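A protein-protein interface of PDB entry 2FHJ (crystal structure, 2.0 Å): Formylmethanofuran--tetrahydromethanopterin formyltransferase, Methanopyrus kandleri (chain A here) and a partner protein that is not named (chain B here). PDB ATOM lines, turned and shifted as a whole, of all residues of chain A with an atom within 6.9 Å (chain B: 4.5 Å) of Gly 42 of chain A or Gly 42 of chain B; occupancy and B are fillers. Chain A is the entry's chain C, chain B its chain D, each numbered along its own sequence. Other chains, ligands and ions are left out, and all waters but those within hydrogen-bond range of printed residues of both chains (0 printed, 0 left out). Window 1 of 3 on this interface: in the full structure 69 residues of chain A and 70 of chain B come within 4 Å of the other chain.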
ATOM      1  N   ALA A  36     -28.002  11.898  14.685  1.00  0.00           N
ATOM      2  CA  ALA A  36     -27.056  11.130  15.500  1.00  0.00           C
ATOM      3  C   ALA A  36     -25.823  11.947  15.844  1.00  0.00           C
ATOM      4  O   ALA A  36     -25.324  11.947  16.983  1.00  0.00           O
ATOM      5  CB  ALA A  36     -26.654   9.865  14.757  1.00  0.00           C
ATOM      6  N   VAL A  37     -25.331  12.631  14.835  1.00  0.00           N
ATOM      7  CA  VAL A  37     -24.151  13.462  14.938  1.00  0.00           C
ATOM      8  C   VAL A  37     -24.317  14.609  15.951  1.00  0.00           C
ATOM      9  O   VAL A  37     -23.437  14.814  16.807  1.00  0.00           O
ATOM     10  CB  VAL A  37     -23.812  14.010  13.534  1.00  0.00           C
ATOM     11  CG1 VAL A  37     -22.879  15.183  13.623  1.00  0.00           C
ATOM     12  CG2 VAL A  37     -23.238  12.892  12.657  1.00  0.00           C
ATOM     13  N   LYS A  38     -25.425  15.352  15.841  1.00  0.00           N
ATOM     14  CA  LYS A  38     -25.711  16.478  16.749  1.00  0.00           C
ATOM     15  C   LYS A  38     -25.826  16.011  18.192  1.00  0.00           C
ATOM     16  O   LYS A  38     -25.347  16.669  19.112  1.00  0.00           O
ATOM     17  CB  LYS A  38     -27.003  17.201  16.347  1.00  0.00           C
ATOM     18  CG  LYS A  38     -26.887  18.030  15.085  1.00  0.00           C
ATOM     19  CD  LYS A  38     -26.184  19.377  15.340  1.00  0.00           C
ATOM     20  CE  LYS A  38     -26.081  20.206  14.063  1.00  0.00           C
ATOM     21  NZ  LYS A  38     -25.256  21.436  14.230  1.00  0.00           N
ATOM     22  N   GLU A  39     -26.446  14.861  18.403  1.00  0.00           N
ATOM     23  CA  GLU A  39     -26.513  14.296  19.743  1.00  0.00           C
ATOM     24  C   GLU A  39     -25.132  13.806  20.187  1.00  0.00           C
ATOM     25  O   GLU A  39     -24.714  14.053  21.325  1.00  0.00           O
ATOM     26  CB  GLU A  39     -27.541  13.164  19.799  1.00  0.00           C
ATOM     27  CG  GLU A  39     -27.797  12.602  21.219  1.00  0.00           C
ATOM     28  CD  GLU A  39     -28.573  13.557  22.128  1.00  0.00           C
ATOM     29  OE1 GLU A  39     -28.275  13.645  23.346  1.00  0.00           O
ATOM     30  OE2 GLU A  39     -29.509  14.233  21.652  1.00  0.00           O
ATOM     31  N   ALA A  40     -24.413  13.117  19.309  1.00  0.00           N
ATOM     32  CA  ALA A  40     -23.082  12.583  19.668  1.00  0.00           C
ATOM     33  C   ALA A  40     -22.032  13.651  19.939  1.00  0.00           C
ATOM     34  O   ALA A  40     -21.173  13.459  20.799  1.00  0.00           O
ATOM     35  CB  ALA A  40     -22.570  11.622  18.600  1.00  0.00           C
ATOM     36  N   THR A  41     -22.111  14.775  19.234  1.00  0.00           N
ATOM     37  CA  THR A  41     -21.122  15.849  19.374  1.00  0.00           C
ATOM     38  C   THR A  41     -21.508  17.009  20.323  1.00  0.00           C
ATOM     39  O   THR A  41     -20.666  17.853  20.637  1.00  0.00           O
ATOM     40  CB  THR A  41     -20.755  16.408  18.002  1.00  0.00           C
ATOM     41  OG1 THR A  41     -21.920  16.971  17.394  1.00  0.00           O
ATOM     42  CG2 THR A  41     -20.182  15.296  17.124  1.00  0.00           C
ATOM     43  N   GLY A  42     -22.758  17.053  20.782  1.00  0.00           N
ATOM     44  CA  GLY A  42     -23.222  18.085  21.693  1.00  0.00           C
ATOM     45  C   GLY A  42     -22.602  17.866  23.058  1.00  0.00           C
ATOM     46  O   GLY A  42     -21.938  16.866  23.253  1.00  0.00           O
ATOM     47  N   PHE A  43     -22.842  18.791  23.984  1.00  0.00           N
ATOM     48  CA  PHE A  43     -22.130  18.881  25.272  1.00  0.00           C
ATOM     49  C   PHE A  43     -20.635  18.615  25.093  1.00  0.00           C
ATOM     50  O   PHE A  43     -20.035  17.817  25.790  1.00  0.00           O
ATOM     51  CB  PHE A  43     -22.787  17.964  26.311  1.00  0.00           C
ATOM     52  CG  PHE A  43     -22.341  18.202  27.749  1.00  0.00           C
ATOM     53  CD1 PHE A  43     -21.986  19.462  28.215  1.00  0.00           C
ATOM     54  CD2 PHE A  43     -22.309  17.146  28.642  1.00  0.00           C
ATOM     55  CE1 PHE A  43     -21.563  19.649  29.542  1.00  0.00           C
ATOM     56  CE2 PHE A  43     -21.916  17.340  29.958  1.00  0.00           C
ATOM     57  CZ  PHE A  43     -21.550  18.596  30.403  1.00  0.00           C
ATOM     58  N   GLY A  44     -20.038  19.302  24.123  1.00  0.00           N
ATOM     59  CA  GLY A  44     -18.653  19.019  23.716  1.00  0.00           C
ATOM     60  C   GLY A  44     -17.989  20.239  23.112  1.00  0.00           C
ATOM     61  O   GLY A  44     -17.612  20.235  21.917  1.00  0.00           O
ATOM     62  N   THR A  45     -17.942  21.315  23.894  1.00  0.00           N
ATOM     63  CA  THR A  45     -17.341  22.556  23.469  1.00  0.00           C
ATOM     64  C   THR A  45     -15.903  22.661  23.964  1.00  0.00           C
ATOM     65  O   THR A  45     -15.020  23.069  23.219  1.00  0.00           O
ATOM     66  CB  THR A  45     -18.157  23.802  23.924  1.00  0.00           C
ATOM     67  OG1 THR A  45     -18.279  23.822  25.347  1.00  0.00           O
ATOM     68  CG2 THR A  45     -19.540  23.792  23.320  1.00  0.00           C
ATOM     69  N   CYS A  50     -16.898  20.417  29.970  1.00  0.00           N
ATOM     70  CA  CYS A  50     -17.543  19.344  29.221  1.00  0.00           C
ATOM     71  C   CYS A  50     -16.682  18.079  29.300  1.00  0.00           C
ATOM     72  O   CYS A  50     -15.482  18.160  29.554  1.00  0.00           O
ATOM     73  CB  CYS A  50     -17.731  19.700  27.751  1.00  0.00           C
ATOM     74  SG  CYS A  50     -18.623  21.196  27.418  1.00  0.00           S
ATOM     75  N   PRO A  51     -17.290  16.910  29.048  1.00  0.00           N
ATOM     76  CA  PRO A  51     -16.547  15.649  29.016  1.00  0.00           C
ATOM     77  C   PRO A  51     -15.690  15.426  27.758  1.00  0.00           C
ATOM     78  O   PRO A  51     -14.894  14.492  27.737  1.00  0.00           O
ATOM     79  CB  PRO A  51     -17.655  14.584  29.094  1.00  0.00           C
ATOM     80  CG  PRO A  51     -18.954  15.339  29.305  1.00  0.00           C
ATOM     81  CD  PRO A  51     -18.723  16.694  28.783  1.00  0.00           C
ATOM     82  N   ALA A  52     -15.861  16.241  26.718  1.00  0.00           N
ATOM     83  CA  ALA A  52     -14.978  16.164  25.547  1.00  0.00           C
ATOM     84  C   ALA A  52     -15.076  17.424  24.705  1.00  0.00           C
ATOM     85  O   ALA A  52     -15.808  18.337  25.048  1.00  0.00           O
ATOM     86  CB  ALA A  52     -15.311  14.945  24.698  1.00  0.00           C
ATOM     87  N   ALA A  54     -15.916  18.021  20.706  1.00  0.00           N
ATOM     88  CA  ALA A  54     -16.415  17.198  19.619  1.00  0.00           C
ATOM     89  C   ALA A  54     -17.094  18.081  18.606  1.00  0.00           C
ATOM     90  O   ALA A  54     -17.557  19.167  18.941  1.00  0.00           O
ATOM     91  CB  ALA A  54     -17.392  16.191  20.156  1.00  0.00           C
ATOM     92  N   GLY A  55     -17.164  17.645  17.366  1.00  0.00           N
ATOM     93  CA  GLY A  55     -17.804  18.489  16.374  1.00  0.00           C
ATOM     94  C   GLY A  55     -17.863  17.790  15.054  1.00  0.00           C
ATOM     95  O   GLY A  55     -17.278  16.733  14.885  1.00  0.00           O
ATOM     96  N   ARG A  92     -20.400   8.160  23.677  1.00  0.00           N
ATOM     97  CA  ARG A  92     -21.130   8.914  22.637  1.00  0.00           C
ATOM     98  C   ARG A  92     -21.575   8.029  21.482  1.00  0.00           C
ATOM     99  O   ARG A  92     -22.617   8.258  20.886  1.00  0.00           O
ATOM    100  CB  ARG A  92     -20.285  10.078  22.122  1.00  0.00           C
ATOM    101  CG  ARG A  92     -20.151  11.241  23.119  1.00  0.00           C
ATOM    102  CD  ARG A  92     -18.933  12.108  22.843  1.00  0.00           C
ATOM    103  NE  ARG A  92     -18.598  12.994  23.965  1.00  0.00           N
ATOM    104  CZ  ARG A  92     -19.107  14.214  24.129  1.00  0.00           C
ATOM    105  NH1 ARG A  92     -18.755  14.963  25.169  1.00  0.00           N
ATOM    106  NH2 ARG A  92     -19.956  14.704  23.250  1.00  0.00           N
ATOM    107  N   CYS A  96     -25.467   7.609  21.833  1.00  0.00           N
ATOM    108  CA  CYS A  96     -25.989   8.592  20.851  1.00  0.00           C
ATOM    109  C   CYS A  96     -26.043   8.123  19.416  1.00  0.00           C
ATOM    110  O   CYS A  96     -26.842   8.655  18.621  1.00  0.00           O
ATOM    111  CB  CYS A  96     -25.165   9.882  20.885  1.00  0.00           C
ATOM    112  SG  CYS A  96     -25.049  10.663  22.513  1.00  0.00           S
ATOM    113  N   LYS B  38     -29.119  22.900  21.075  1.00  0.00           N
ATOM    114  CA  LYS B  38     -28.604  21.625  20.574  1.00  0.00           C
ATOM    115  C   LYS B  38     -27.294  21.241  21.249  1.00  0.00           C
ATOM    116  O   LYS B  38     -27.081  20.070  21.597  1.00  0.00           O
ATOM    117  CB  LYS B  38     -28.405  21.676  19.065  1.00  0.00           C
ATOM    118  CG  LYS B  38     -29.706  21.694  18.286  1.00  0.00           C
ATOM    119  CD  LYS B  38     -30.346  20.317  18.228  1.00  0.00           C
ATOM    120  CE  LYS B  38     -31.762  20.386  17.671  1.00  0.00           C
ATOM    121  NZ  LYS B  38     -32.606  19.233  18.101  1.00  0.00           N
ATOM    122  N   GLU B  39     -26.415  22.219  21.436  1.00  0.00           N
ATOM    123  CA  GLU B  39     -25.162  21.955  22.132  1.00  0.00           C
ATOM    124  C   GLU B  39     -25.429  21.649  23.598  1.00  0.00           C
ATOM    125  O   GLU B  39     -24.888  20.696  24.146  1.00  0.00           O
ATOM    126  CB  GLU B  39     -24.194  23.127  21.965  1.00  0.00           C
ATOM    127  CG  GLU B  39     -22.783  22.873  22.539  1.00  0.00           C
ATOM    128  CD  GLU B  39     -21.957  21.898  21.742  1.00  0.00           C
ATOM    129  OE1 GLU B  39     -21.193  21.129  22.374  1.00  0.00           O
ATOM    130  OE2 GLU B  39     -22.046  21.895  20.490  1.00  0.00           O
ATOM    131  N   ALA B  40     -26.279  22.438  24.235  1.00  0.00           N
ATOM    132  CA  ALA B  40     -26.576  22.247  25.671  1.00  0.00           C
ATOM    133  C   ALA B  40     -27.314  20.952  25.992  1.00  0.00           C
ATOM    134  O   ALA B  40     -27.141  20.404  27.074  1.00  0.00           O
ATOM    135  CB  ALA B  40     -27.357  23.417  26.217  1.00  0.00           C
ATOM    136  N   THR B  41     -28.137  20.469  25.065  1.00  0.00           N
ATOM    137  CA  THR B  41     -28.940  19.265  25.296  1.00  0.00           C
ATOM    138  C   THR B  41     -28.395  17.971  24.668  1.00  0.00           C
ATOM    139  O   THR B  41     -28.914  16.897  24.974  1.00  0.00           O
ATOM    140  CB  THR B  41     -30.378  19.464  24.828  1.00  0.00           C
ATOM    141  OG1 THR B  41     -30.387  19.763  23.429  1.00  0.00           O
ATOM    142  CG2 THR B  41     -31.016  20.603  25.595  1.00  0.00           C
ATOM    143  N   GLY B  42     -27.363  18.058  23.818  1.00  0.00           N
ATOM    144  CA  GLY B  42     -26.711  16.873  23.233  1.00  0.00           C
ATOM    145  C   GLY B  42     -25.950  16.111  24.312  1.00  0.00           C
ATOM    146  O   GLY B  42     -25.897  16.574  25.437  1.00  0.00           O
ATOM    147  N   PHE B  43     -25.363  14.966  23.949  1.00  0.00           N
ATOM    148  CA  PHE B  43     -24.783  13.975  24.892  1.00  0.00           C
ATOM    149  C   PHE B  43     -25.669  13.840  26.135  1.00  0.00           C
ATOM    150  O   PHE B  43     -25.210  13.912  27.264  1.00  0.00           O
ATOM    151  CB  PHE B  43     -23.313  14.323  25.226  1.00  0.00           C
ATOM    152  CG  PHE B  43     -22.524  13.212  25.938  1.00  0.00           C
ATOM    153  CD1 PHE B  43     -22.754  11.873  25.685  1.00  0.00           C
ATOM    154  CD2 PHE B  43     -21.521  13.549  26.838  1.00  0.00           C
ATOM    155  CE1 PHE B  43     -22.019  10.879  26.333  1.00  0.00           C
ATOM    156  CE2 PHE B  43     -20.777  12.561  27.507  1.00  0.00           C
ATOM    157  CZ  PHE B  43     -21.028  11.227  27.244  1.00  0.00           C
ATOM    158  N   GLY B  44     -26.965  13.644  25.899  1.00  0.00           N
ATOM    159  CA  GLY B  44     -27.948  13.654  26.974  1.00  0.00           C
ATOM    160  C   GLY B  44     -29.176  12.810  26.688  1.00  0.00           C
ATOM    161  O   GLY B  44     -30.302  13.310  26.717  1.00  0.00           O
ATOM    162  N   ARG B  92     -23.586  22.657  31.481  1.00  0.00           N
ATOM    163  CA  ARG B  92     -24.229  22.849  30.175  1.00  0.00           C
ATOM    164  C   ARG B  92     -24.596  24.304  29.909  1.00  0.00           C
ATOM    165  O   ARG B  92     -24.554  24.757  28.764  1.00  0.00           O
ATOM    166  CB  ARG B  92     -25.468  21.964  30.045  1.00  0.00           C
ATOM    167  CG  ARG B  92     -25.161  20.477  29.821  1.00  0.00           C
ATOM    168  CD  ARG B  92     -26.339  19.576  30.194  1.00  0.00           C
ATOM    169  NE  ARG B  92     -25.959  18.164  30.335  1.00  0.00           N
ATOM    170  CZ  ARG B  92     -25.914  17.292  29.333  1.00  0.00           C
ATOM    171  NH1 ARG B  92     -25.560  16.034  29.547  1.00  0.00           N
ATOM    172  NH2 ARG B  92     -26.227  17.656  28.105  1.00  0.00           N
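The backbone carbonyl oxygen (O) of Glu 39 of chain A is in hydrogen-bond range of the backbone NH (N) of Phe 43 of chain B.
N of Gly 44 of chain B sits at hydrogen-bond distance from OE1 of Glu 39 of chain A, at 2.9 Å.
The backbone NH (N) of Phe 43 of chain A sits at hydrogen-bond distance from the backbone carbonyl oxygen (O) of Glu 39 of chain B, 2.8 Å away.
The backbone NH of Gly 44 of chain A lies within hydrogen-bond range of the side-chain carboxylate of Glu 39 of chain B (2.8 Å).
O of Val 37 of chain A lies within hydrogen-bond range of OG1 of Thr 41 of chain A, 2.7 Å away.
The side-chain sulfur of Cys 96 of chain A sits close to the backbone carbonyl oxygen of Glu 39 of chain A (3.6 Å).
The guanidinium group of Arg 92 of chain A lies within hydrogen-bond range of the backbone carbonyl oxygen of Gly 42 of chain A.
NH2 of Arg 92 of chain B sits at hydrogen-bond distance from O of Ala 40 of chain B, 3.1 Å away.
O of Gly 42 of chain B is in hydrogen-bond range of NH2 of Arg 92 of chain B (2.9 Å).
O of Phe 43 of chain B lies within hydrogen-bond range of NH1 of Arg 92 of chain B (3.1 Å).
Among the printed residues, pairs that only touch across the chains: Thr 45 of chain A with Glu 39 of chain B, Gly 42 of chain A with Phe 43 of chain B, Phe 43 of chain A with Gly 42 of chain B, Glu 39 of chain A with Gly 42 of chain B, Arg 92 of chain A with Phe 43 of chain B, Phe 43 of chain A with Arg 92 of chain B, Gly 42 of chain A with Glu 39 of chain B, Glu 39 of chain A with Thr 41 of chain B, Thr 41 of chain A with Glu 39 of chain B, Pro 51 of chain A with Phe 43 of chain B, Phe 43 of chain A with Phe 43 of chain B and Gly 42 of chain A with Gly 42 of chain B.
Printed residues of chain A within 4 Å of Gly 42 of chain B: Glu 39 (3.5 Å), Gly 42 (3.98 Å) and Phe 43 (3.5 Å).
Printed residues of chain B within 4 Å of Thr 45 of chain A: Glu 39 (3.3 Å).
Printed residues of chain A within 4 Å of Gly 44 of chain B: Glu 39 (2.9 Å).
Ala 36 of chain A touches none of the printed residues of chain B.
The nearest printed residue of chain B that does not touch Gly 42 of chain A is Lys 38 of chain B (4.3 Å).
The nearest printed residue of chain A that does not touch Gly 44 of chain B is Cys 96 of chain A (4.9 Å).
Printed residues of chain B that touch a printed residue of chain A: Glu 39, Thr 41, Gly 42, Phe 43, Gly 44 and Arg 92.
Among the printed residues, 16 pairs touch across the chains.
Among the printed residues, no Asp or Glu carboxylate lies within 4 Å of a Lys or Arg side-chain nitrogen of the other chain.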
